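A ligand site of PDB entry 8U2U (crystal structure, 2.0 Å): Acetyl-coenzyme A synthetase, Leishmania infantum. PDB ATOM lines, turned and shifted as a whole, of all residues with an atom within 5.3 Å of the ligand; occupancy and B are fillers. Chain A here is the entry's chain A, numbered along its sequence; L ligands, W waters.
N4 of the ligand lies close to O of Glu 448, at 3.4 Å. Merely in contact with the ligand: Ile 370 (3.8 Å), Pro 449 (3.3 Å), Trp 473 (3.6 Å), Trp 474 (3.5 Å) and Ile 572 (3.5 Å). Hydrophobic or aromatic side chains within 4 Å of the ligand: Ile 370, Pro 449, Trp 473 and Ile 572. Within 4 Å of the ligand: Ile 370, Gly 447, Glu 448, Pro 449, Asp 471, Thr 472, Trp 473, Trp 474, Gln 475, Thr 476, Asp 560, Ile 572, Arg 575, Asn 581 and Arg 586. Along chain A the residues within 4 Å of the ligand span positions 370 to 586. The nearest printed residue that does not touch the ligand is Glu 477 (4.3 Å).
The backbone NH (N) of Asp 560 lies within hydrogen-bond range of the side-chain hydroxyl (OG1) of Thr 558 (3.0 Å). The side-chain amide nitrogen (NE2) of Gln 475 sits at hydrogen-bond distance from the backbone carbonyl oxygen (O) of Thr 558 (2.9 Å). The guanidinium group of Arg 586 lies within salt-bridge range of the side-chain carboxylate of Glu 477 (2.7 Å). The side-chain carboxylate (OD1) of Asp 560 sits close to the backbone NH (N) of Arg 575, 3.4 Å away. The backbone NH of Thr 472 sits at hydrogen-bond distance from the backbone carbonyl oxygen of Ser 445 (3.1 Å). OE2 of Glu 448 is in hydrogen-bond range of N of Gly 584. OD2 of Asp 560 lies within hydrogen-bond range of NE1 of Trp 473 (3.0 Å).
A nitrogen (N2) of the ligand is in hydrogen-bond range of the backbone NH of Gly 447 (3.1 Å). N of Thr 476 lies within hydrogen-bond range of O3 of the ligand (2.8 Å). The guanidinium group of Arg 575 lies within hydrogen-bond range of an oxygen (O6) of the ligand (3.1 Å). The guanidinium group (NH2) of Arg 586 is in salt-bridge range of an oxygen (O3) of the ligand (2.8 Å). The side-chain carboxylate (OD1) of Asp 471 is in hydrogen-bond range of a nitrogen (N3) of the ligand (3.0 Å). O of Thr 472 is in hydrogen-bond range of N3 of the ligand, 2.9 Å away. OG1 of Thr 476 sits at hydrogen-bond distance from O3 of the ligand (2.7 Å). The side-chain amide nitrogen of Gln 475 lies within hydrogen-bond range of an oxygen (O6) of the ligand (3.1 Å). The side-chain amide nitrogen (ND2) of Asn 581 sits at hydrogen-bond distance from an oxygen (O7) of the ligand (2.9 Å). The side-chain carboxylate (OD2) of Asp 560 lies within hydrogen-bond range of an oxygen (O6) of the ligand (2.6 Å).
Water W1 lies within hydrogen-bond range of a nitrogen (N4) of the ligand (2.8 Å) and the side-chain carboxylate (OD2) of Asp 471 (2.9 Å).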
ATOM      1  N   THR A 324       7.982   6.358  -8.354  1.00  0.00           N
ATOM      2  CA  THR A 324       7.713   6.936  -7.044  1.00  0.00           C
ATOM      3  C   THR A 324       8.987   7.565  -6.507  1.00  0.00           C
ATOM      4  O   THR A 324      10.083   7.021  -6.723  1.00  0.00           O
ATOM      5  CB  THR A 324       7.196   5.880  -6.051  1.00  0.00           C
ATOM      6  OG1 THR A 324       6.184   5.073  -6.668  1.00  0.00           O
ATOM      7  CG2 THR A 324       6.614   6.560  -4.782  1.00  0.00           C
ATOM      8  N   ILE A 370      -0.954   5.825  -7.450  1.00  0.00           N
ATOM      9  CA  ILE A 370      -1.432   4.505  -7.058  1.00  0.00           C
ATOM     10  C   ILE A 370      -2.891   4.553  -6.643  1.00  0.00           C
ATOM     11  O   ILE A 370      -3.638   3.592  -6.856  1.00  0.00           O
ATOM     12  CB  ILE A 370      -0.539   3.922  -5.948  1.00  0.00           C
ATOM     13  CG1 ILE A 370      -0.883   2.447  -5.722  1.00  0.00           C
ATOM     14  CG2 ILE A 370      -0.588   4.766  -4.672  1.00  0.00           C
ATOM     15  CD1 ILE A 370      -0.300   1.517  -6.801  1.00  0.00           C
ATOM     16  N   THR A 371      -3.330   5.664  -6.042  1.00  0.00           N
ATOM     17  CA  THR A 371      -4.733   5.738  -5.651  1.00  0.00           C
ATOM     18  C   THR A 371      -5.667   5.523  -6.830  1.00  0.00           C
ATOM     19  O   THR A 371      -6.705   4.860  -6.687  1.00  0.00           O
ATOM     20  CB  THR A 371      -5.014   7.081  -5.000  1.00  0.00           C
ATOM     21  OG1 THR A 371      -4.113   7.280  -3.904  1.00  0.00           O
ATOM     22  CG2 THR A 371      -6.440   7.101  -4.501  1.00  0.00           C
ATOM     23  N   SER A 445     -10.469   9.481   3.048  1.00  0.00           N
ATOM     24  CA  SER A 445      -9.386  10.450   3.026  1.00  0.00           C
ATOM     25  C   SER A 445      -8.081   9.712   2.754  1.00  0.00           C
ATOM     26  O   SER A 445      -7.796   8.694   3.396  1.00  0.00           O
ATOM     27  CB  SER A 445      -9.294  11.206   4.355  1.00  0.00           C
ATOM     28  OG  SER A 445      -8.389  12.272   4.224  1.00  0.00           O
ATOM     29  N   VAL A 446      -7.286  10.228   1.818  1.00  0.00           N
ATOM     30  CA  VAL A 446      -6.055   9.552   1.432  1.00  0.00           C
ATOM     31  C   VAL A 446      -4.919  10.502   1.082  1.00  0.00           C
ATOM     32  O   VAL A 446      -5.122  11.566   0.493  1.00  0.00           O
ATOM     33  CB  VAL A 446      -6.294   8.638   0.212  1.00  0.00           C
ATOM     34  CG1 VAL A 446      -6.772   9.461  -0.985  1.00  0.00           C
ATOM     35  CG2 VAL A 446      -5.054   7.866  -0.107  1.00  0.00           C
ATOM     36  N   GLY A 447      -3.716  10.109   1.472  1.00  0.00           N
ATOM     37  CA  GLY A 447      -2.504  10.639   0.889  1.00  0.00           C
ATOM     38  C   GLY A 447      -1.658  11.459   1.822  1.00  0.00           C
ATOM     39  O   GLY A 447      -0.496  11.733   1.497  1.00  0.00           O
ATOM     40  N   GLU A 448      -2.212  11.872   2.951  1.00  0.00           N
ATOM     41  CA  GLU A 448      -1.545  12.733   3.908  1.00  0.00           C
ATOM     42  C   GLU A 448      -2.373  12.693   5.177  1.00  0.00           C
ATOM     43  O   GLU A 448      -3.510  12.232   5.139  1.00  0.00           O
ATOM     44  CB  GLU A 448      -1.431  14.172   3.386  1.00  0.00           C
ATOM     45  CG  GLU A 448      -2.768  14.683   2.857  1.00  0.00           C
ATOM     46  CD  GLU A 448      -2.698  16.088   2.276  1.00  0.00           C
ATOM     47  OE1 GLU A 448      -2.035  16.938   2.896  1.00  0.00           O
ATOM     48  OE2 GLU A 448      -3.320  16.330   1.196  1.00  0.00           O
ATOM     49  N   PRO A 449      -1.822  13.141   6.287  1.00  0.00           N
ATOM     50  CA  PRO A 449      -2.613  13.171   7.519  1.00  0.00           C
ATOM     51  C   PRO A 449      -3.726  14.201   7.387  1.00  0.00           C
ATOM     52  O   PRO A 449      -3.581  15.211   6.692  1.00  0.00           O
ATOM     53  CB  PRO A 449      -1.582  13.583   8.575  1.00  0.00           C
ATOM     54  CG  PRO A 449      -0.236  13.447   7.905  1.00  0.00           C
ATOM     55  CD  PRO A 449      -0.484  13.710   6.467  1.00  0.00           C
ATOM     56  N   ASP A 471     -10.259   7.147   6.989  1.00  0.00           N
ATOM     57  CA  ASP A 471      -8.887   7.673   6.850  1.00  0.00           C
ATOM     58  C   ASP A 471      -7.933   6.500   6.593  1.00  0.00           C
ATOM     59  O   ASP A 471      -7.583   5.745   7.505  1.00  0.00           O
ATOM     60  CB  ASP A 471      -8.522   8.451   8.128  1.00  0.00           C
ATOM     61  CG  ASP A 471      -7.110   9.012   8.093  1.00  0.00           C
ATOM     62  OD1 ASP A 471      -6.464   8.925   7.011  1.00  0.00           O
ATOM     63  OD2 ASP A 471      -6.658   9.547   9.126  1.00  0.00           O
ATOM     64  N   THR A 472      -7.513   6.319   5.339  1.00  0.00           N
ATOM     65  CA  THR A 472      -6.822   5.106   4.910  1.00  0.00           C
ATOM     66  C   THR A 472      -5.339   5.412   4.822  1.00  0.00           C
ATOM     67  O   THR A 472      -4.944   6.181   3.955  1.00  0.00           O
ATOM     68  CB  THR A 472      -7.286   4.643   3.523  1.00  0.00           C
ATOM     69  OG1 THR A 472      -7.028   5.670   2.556  1.00  0.00           O
ATOM     70  CG2 THR A 472      -8.738   4.297   3.475  1.00  0.00           C
ATOM     71  N   TRP A 473      -4.508   4.746   5.622  1.00  0.00           N
ATOM     72  CA  TRP A 473      -3.065   4.902   5.453  1.00  0.00           C
ATOM     73  C   TRP A 473      -2.529   3.782   4.567  1.00  0.00           C
ATOM     74  O   TRP A 473      -2.884   2.610   4.759  1.00  0.00           O
ATOM     75  CB  TRP A 473      -2.290   4.932   6.778  1.00  0.00           C
ATOM     76  CG  TRP A 473      -0.829   4.997   6.470  1.00  0.00           C
ATOM     77  CD1 TRP A 473      -0.108   6.117   6.204  1.00  0.00           C
ATOM     78  CD2 TRP A 473       0.064   3.903   6.309  1.00  0.00           C
ATOM     79  NE1 TRP A 473       1.185   5.795   5.933  1.00  0.00           N
ATOM     80  CE2 TRP A 473       1.322   4.433   5.970  1.00  0.00           C
ATOM     81  CE3 TRP A 473      -0.073   2.509   6.410  1.00  0.00           C
ATOM     82  CZ2 TRP A 473       2.436   3.628   5.712  1.00  0.00           C
ATOM     83  CZ3 TRP A 473       1.045   1.702   6.166  1.00  0.00           C
ATOM     84  CH2 TRP A 473       2.290   2.273   5.820  1.00  0.00           C
ATOM     85  N   TRP A 474      -1.704   4.145   3.599  1.00  0.00           N
ATOM     86  CA  TRP A 474      -0.974   3.159   2.786  1.00  0.00           C
ATOM     87  C   TRP A 474      -0.005   3.945   1.886  1.00  0.00           C
ATOM     88  O   TRP A 474       0.187   5.152   2.042  1.00  0.00           O
ATOM     89  CB  TRP A 474      -1.941   2.269   1.996  1.00  0.00           C
ATOM     90  CG  TRP A 474      -2.816   3.060   1.068  1.00  0.00           C
ATOM     91  CD1 TRP A 474      -3.707   4.063   1.407  1.00  0.00           C
ATOM     92  CD2 TRP A 474      -2.889   2.931  -0.376  1.00  0.00           C
ATOM     93  NE1 TRP A 474      -4.335   4.535   0.269  1.00  0.00           N
ATOM     94  CE2 TRP A 474      -3.844   3.872  -0.831  1.00  0.00           C
ATOM     95  CE3 TRP A 474      -2.258   2.101  -1.308  1.00  0.00           C
ATOM     96  CZ2 TRP A 474      -4.153   4.008  -2.183  1.00  0.00           C
ATOM     97  CZ3 TRP A 474      -2.583   2.246  -2.648  1.00  0.00           C
ATOM     98  CH2 TRP A 474      -3.537   3.187  -3.067  1.00  0.00           C
ATOM     99  N   GLN A 475       0.643   3.231   0.963  1.00  0.00           N
ATOM    100  CA  GLN A 475       1.639   3.855   0.089  1.00  0.00           C
ATOM    101  C   GLN A 475       1.708   3.044  -1.210  1.00  0.00           C
ATOM    102  O   GLN A 475       1.238   1.910  -1.288  1.00  0.00           O
ATOM    103  CB  GLN A 475       3.028   3.966   0.766  1.00  0.00           C
ATOM    104  CG  GLN A 475       3.355   2.779   1.699  1.00  0.00           C
ATOM    105  CD  GLN A 475       4.657   2.893   2.506  1.00  0.00           C
ATOM    106  OE1 GLN A 475       5.240   1.882   2.869  1.00  0.00           O
ATOM    107  NE2 GLN A 475       5.068   4.095   2.823  1.00  0.00           N
ATOM    108  N   THR A 476       2.294   3.663  -2.226  1.00  0.00           N
ATOM    109  CA  THR A 476       2.522   2.960  -3.498  1.00  0.00           C
ATOM    110  C   THR A 476       3.008   1.533  -3.285  1.00  0.00           C
ATOM    111  O   THR A 476       2.478   0.576  -3.875  1.00  0.00           O
ATOM    112  CB  THR A 476       3.539   3.743  -4.315  1.00  0.00           C
ATOM    113  OG1 THR A 476       3.076   5.078  -4.536  1.00  0.00           O
ATOM    114  CG2 THR A 476       3.795   3.092  -5.703  1.00  0.00           C
ATOM    115  N   GLU A 477       3.997   1.363  -2.419  1.00  0.00           N
ATOM    116  CA  GLU A 477       4.628   0.073  -2.194  1.00  0.00           C
ATOM    117  C   GLU A 477       3.716  -0.974  -1.549  1.00  0.00           C
ATOM    118  O   GLU A 477       4.087  -2.157  -1.559  1.00  0.00           O
ATOM    119  CB  GLU A 477       5.873   0.242  -1.317  1.00  0.00           C
ATOM    120  CG  GLU A 477       6.934   1.139  -1.912  1.00  0.00           C
ATOM    121  CD  GLU A 477       6.835   2.576  -1.415  1.00  0.00           C
ATOM    122  OE1 GLU A 477       5.719   3.040  -1.175  1.00  0.00           O
ATOM    123  OE2 GLU A 477       7.877   3.249  -1.302  1.00  0.00           O
ATOM    124  N   THR A 558       8.308   1.220   6.411  1.00  0.00           N
ATOM    125  CA  THR A 558       7.398   2.054   5.627  1.00  0.00           C
ATOM    126  C   THR A 558       8.009   3.381   5.220  1.00  0.00           C
ATOM    127  O   THR A 558       7.544   3.994   4.266  1.00  0.00           O
ATOM    128  CB  THR A 558       6.110   2.342   6.410  1.00  0.00           C
ATOM    129  OG1 THR A 558       6.424   3.147   7.550  1.00  0.00           O
ATOM    130  CG2 THR A 558       5.421   1.081   6.850  1.00  0.00           C
ATOM    131  N   ASP A 560       7.551   5.856   7.196  1.00  0.00           N
ATOM    132  CA  ASP A 560       6.715   6.774   7.973  1.00  0.00           C
ATOM    133  C   ASP A 560       6.980   6.617   9.471  1.00  0.00           C
ATOM    134  O   ASP A 560       7.352   5.539   9.954  1.00  0.00           O
ATOM    135  CB  ASP A 560       5.226   6.527   7.726  1.00  0.00           C
ATOM    136  CG  ASP A 560       4.773   7.096   6.406  1.00  0.00           C
ATOM    137  OD1 ASP A 560       5.060   8.283   6.151  1.00  0.00           O
ATOM    138  OD2 ASP A 560       4.143   6.364   5.616  1.00  0.00           O
ATOM    139  N   ILE A 572      -0.488   8.303  12.155  1.00  0.00           N
ATOM    140  CA  ILE A 572       0.667   8.452  11.292  1.00  0.00           C
ATOM    141  C   ILE A 572       1.152   9.896  11.322  1.00  0.00           C
ATOM    142  O   ILE A 572       0.388  10.825  11.063  1.00  0.00           O
ATOM    143  CB  ILE A 572       0.358   7.995   9.857  1.00  0.00           C
ATOM    144  CG1 ILE A 572       0.403   6.477   9.786  1.00  0.00           C
ATOM    145  CG2 ILE A 572       1.433   8.552   8.891  1.00  0.00           C
ATOM    146  CD1 ILE A 572      -0.835   5.823  10.113  1.00  0.00           C
ATOM    147  N   GLY A 574       3.989  11.091   9.631  1.00  0.00           N
ATOM    148  CA  GLY A 574       4.586  11.566   8.407  1.00  0.00           C
ATOM    149  C   GLY A 574       5.933  10.919   8.166  1.00  0.00           C
ATOM    150  O   GLY A 574       6.418  10.112   8.954  1.00  0.00           O
ATOM    151  N   ARG A 575       6.512  11.279   7.012  1.00  0.00           N
ATOM    152  CA  ARG A 575       7.756  10.686   6.538  1.00  0.00           C
ATOM    153  C   ARG A 575       8.908  10.986   7.480  1.00  0.00           C
ATOM    154  O   ARG A 575       9.047  12.110   7.981  1.00  0.00           O
ATOM    155  CB  ARG A 575       8.113  11.211   5.140  1.00  0.00           C
ATOM    156  CG  ARG A 575       7.074  10.917   4.092  1.00  0.00           C
ATOM    157  CD  ARG A 575       6.972   9.432   3.738  1.00  0.00           C
ATOM    158  NE  ARG A 575       8.197   8.861   3.190  1.00  0.00           N
ATOM    159  CZ  ARG A 575       8.251   7.710   2.541  1.00  0.00           C
ATOM    160  NH1 ARG A 575       7.159   7.051   2.200  1.00  0.00           N
ATOM    161  NH2 ARG A 575       9.440   7.206   2.199  1.00  0.00           N
ATOM    162  N   ASN A 581       5.369  15.295   1.318  1.00  0.00           N
ATOM    163  CA  ASN A 581       4.010  15.020   0.856  1.00  0.00           C
ATOM    164  C   ASN A 581       3.366  16.374   0.663  1.00  0.00           C
ATOM    165  O   ASN A 581       2.952  17.018   1.634  1.00  0.00           O
ATOM    166  CB  ASN A 581       3.208  14.178   1.836  1.00  0.00           C
ATOM    167  CG  ASN A 581       3.328  12.720   1.566  1.00  0.00           C
ATOM    168  OD1 ASN A 581       3.009  12.226   0.450  1.00  0.00           O
ATOM    169  ND2 ASN A 581       3.784  11.987   2.574  1.00  0.00           N
ATOM    170  N   GLY A 584      -0.660  16.036  -0.817  1.00  0.00           N
ATOM    171  CA  GLY A 584      -0.865  14.619  -0.965  1.00  0.00           C
ATOM    172  C   GLY A 584       0.090  13.920  -1.919  1.00  0.00           C
ATOM    173  O   GLY A 584       0.029  12.687  -2.034  1.00  0.00           O
ATOM    174  N   ARG A 586       3.717  12.624  -3.057  1.00  0.00           N
ATOM    175  CA  ARG A 586       5.070  12.275  -2.637  1.00  0.00           C
ATOM    176  C   ARG A 586       6.114  12.780  -3.638  1.00  0.00           C
ATOM    177  O   ARG A 586       6.035  12.473  -4.823  1.00  0.00           O
ATOM    178  CB  ARG A 586       5.180  10.745  -2.519  1.00  0.00           C
ATOM    179  CG  ARG A 586       6.291  10.349  -1.583  1.00  0.00           C
ATOM    180  CD  ARG A 586       6.989   9.087  -1.982  1.00  0.00           C
ATOM    181  NE  ARG A 586       6.166   7.920  -1.779  1.00  0.00           N
ATOM    182  CZ  ARG A 586       6.637   6.707  -1.531  1.00  0.00           C
ATOM    183  NH1 ARG A 586       7.935   6.477  -1.384  1.00  0.00           N
ATOM    184  NH2 ARG A 586       5.789   5.690  -1.444  1.00  0.00           N
HETATM  185  P1  LIG L   1       2.255   7.526  -2.183  1.00  0.00           P
HETATM  186  O1  LIG L   1       2.401   8.556  -3.256  1.00  0.00           O
HETATM  187  O2  LIG L   1       0.826   7.054  -2.054  1.00  0.00           O
HETATM  188  O3  LIG L   1       3.197   6.350  -2.190  1.00  0.00           O
HETATM  189  O4  LIG L   1       2.577   8.293  -0.831  1.00  0.00           O
HETATM  190  C1  LIG L   1       2.649   7.533   0.370  1.00  0.00           C
HETATM  191  C2  LIG L   1       2.864   8.392   1.582  1.00  0.00           C
HETATM  192  O5  LIG L   1       1.737   9.294   1.759  1.00  0.00           O
HETATM  193  C3  LIG L   1       2.946   7.638   2.891  1.00  0.00           C
HETATM  194  O6  LIG L   1       4.226   7.076   3.091  1.00  0.00           O
HETATM  195  C4  LIG L   1       2.553   8.703   3.913  1.00  0.00           C
HETATM  196  O7  LIG L   1       3.639   9.560   4.228  1.00  0.00           O
HETATM  197  C5  LIG L   1       1.513   9.506   3.140  1.00  0.00           C
HETATM  198  N1  LIG L   1       0.139   9.086   3.445  1.00  0.00           N
HETATM  199  C6  LIG L   1      -0.709   8.461   2.593  1.00  0.00           C
HETATM  200  N2  LIG L   1      -1.902   8.240   3.202  1.00  0.00           N
HETATM  201  C7  LIG L   1      -1.814   8.770   4.455  1.00  0.00           C
HETATM  202  C8  LIG L   1      -2.707   8.901   5.605  1.00  0.00           C
HETATM  203  N3  LIG L   1      -3.954   8.397   5.500  1.00  0.00           N
HETATM  204  N4  LIG L   1      -2.241   9.486   6.736  1.00  0.00           N
HETATM  205  C9  LIG L   1      -0.988   9.976   6.802  1.00  0.00           C
HETATM  206  N5  LIG L   1      -0.122   9.905   5.759  1.00  0.00           N
HETATM  207  C10 LIG L   1      -0.475   9.327   4.604  1.00  0.00           C
HETATM  208  O   HOH W   1      -3.882   8.746   8.939  1.00  0.00           O
HETATM  209  O   HOH W   2      -0.863   8.770  -1.195  1.00  0.00           O
HETATM  210  O   HOH W   3       2.274  11.229   5.978  1.00  0.00           O
HETATM  211  O   HOH W   4       4.158   8.515  -5.299  1.00  0.00           O
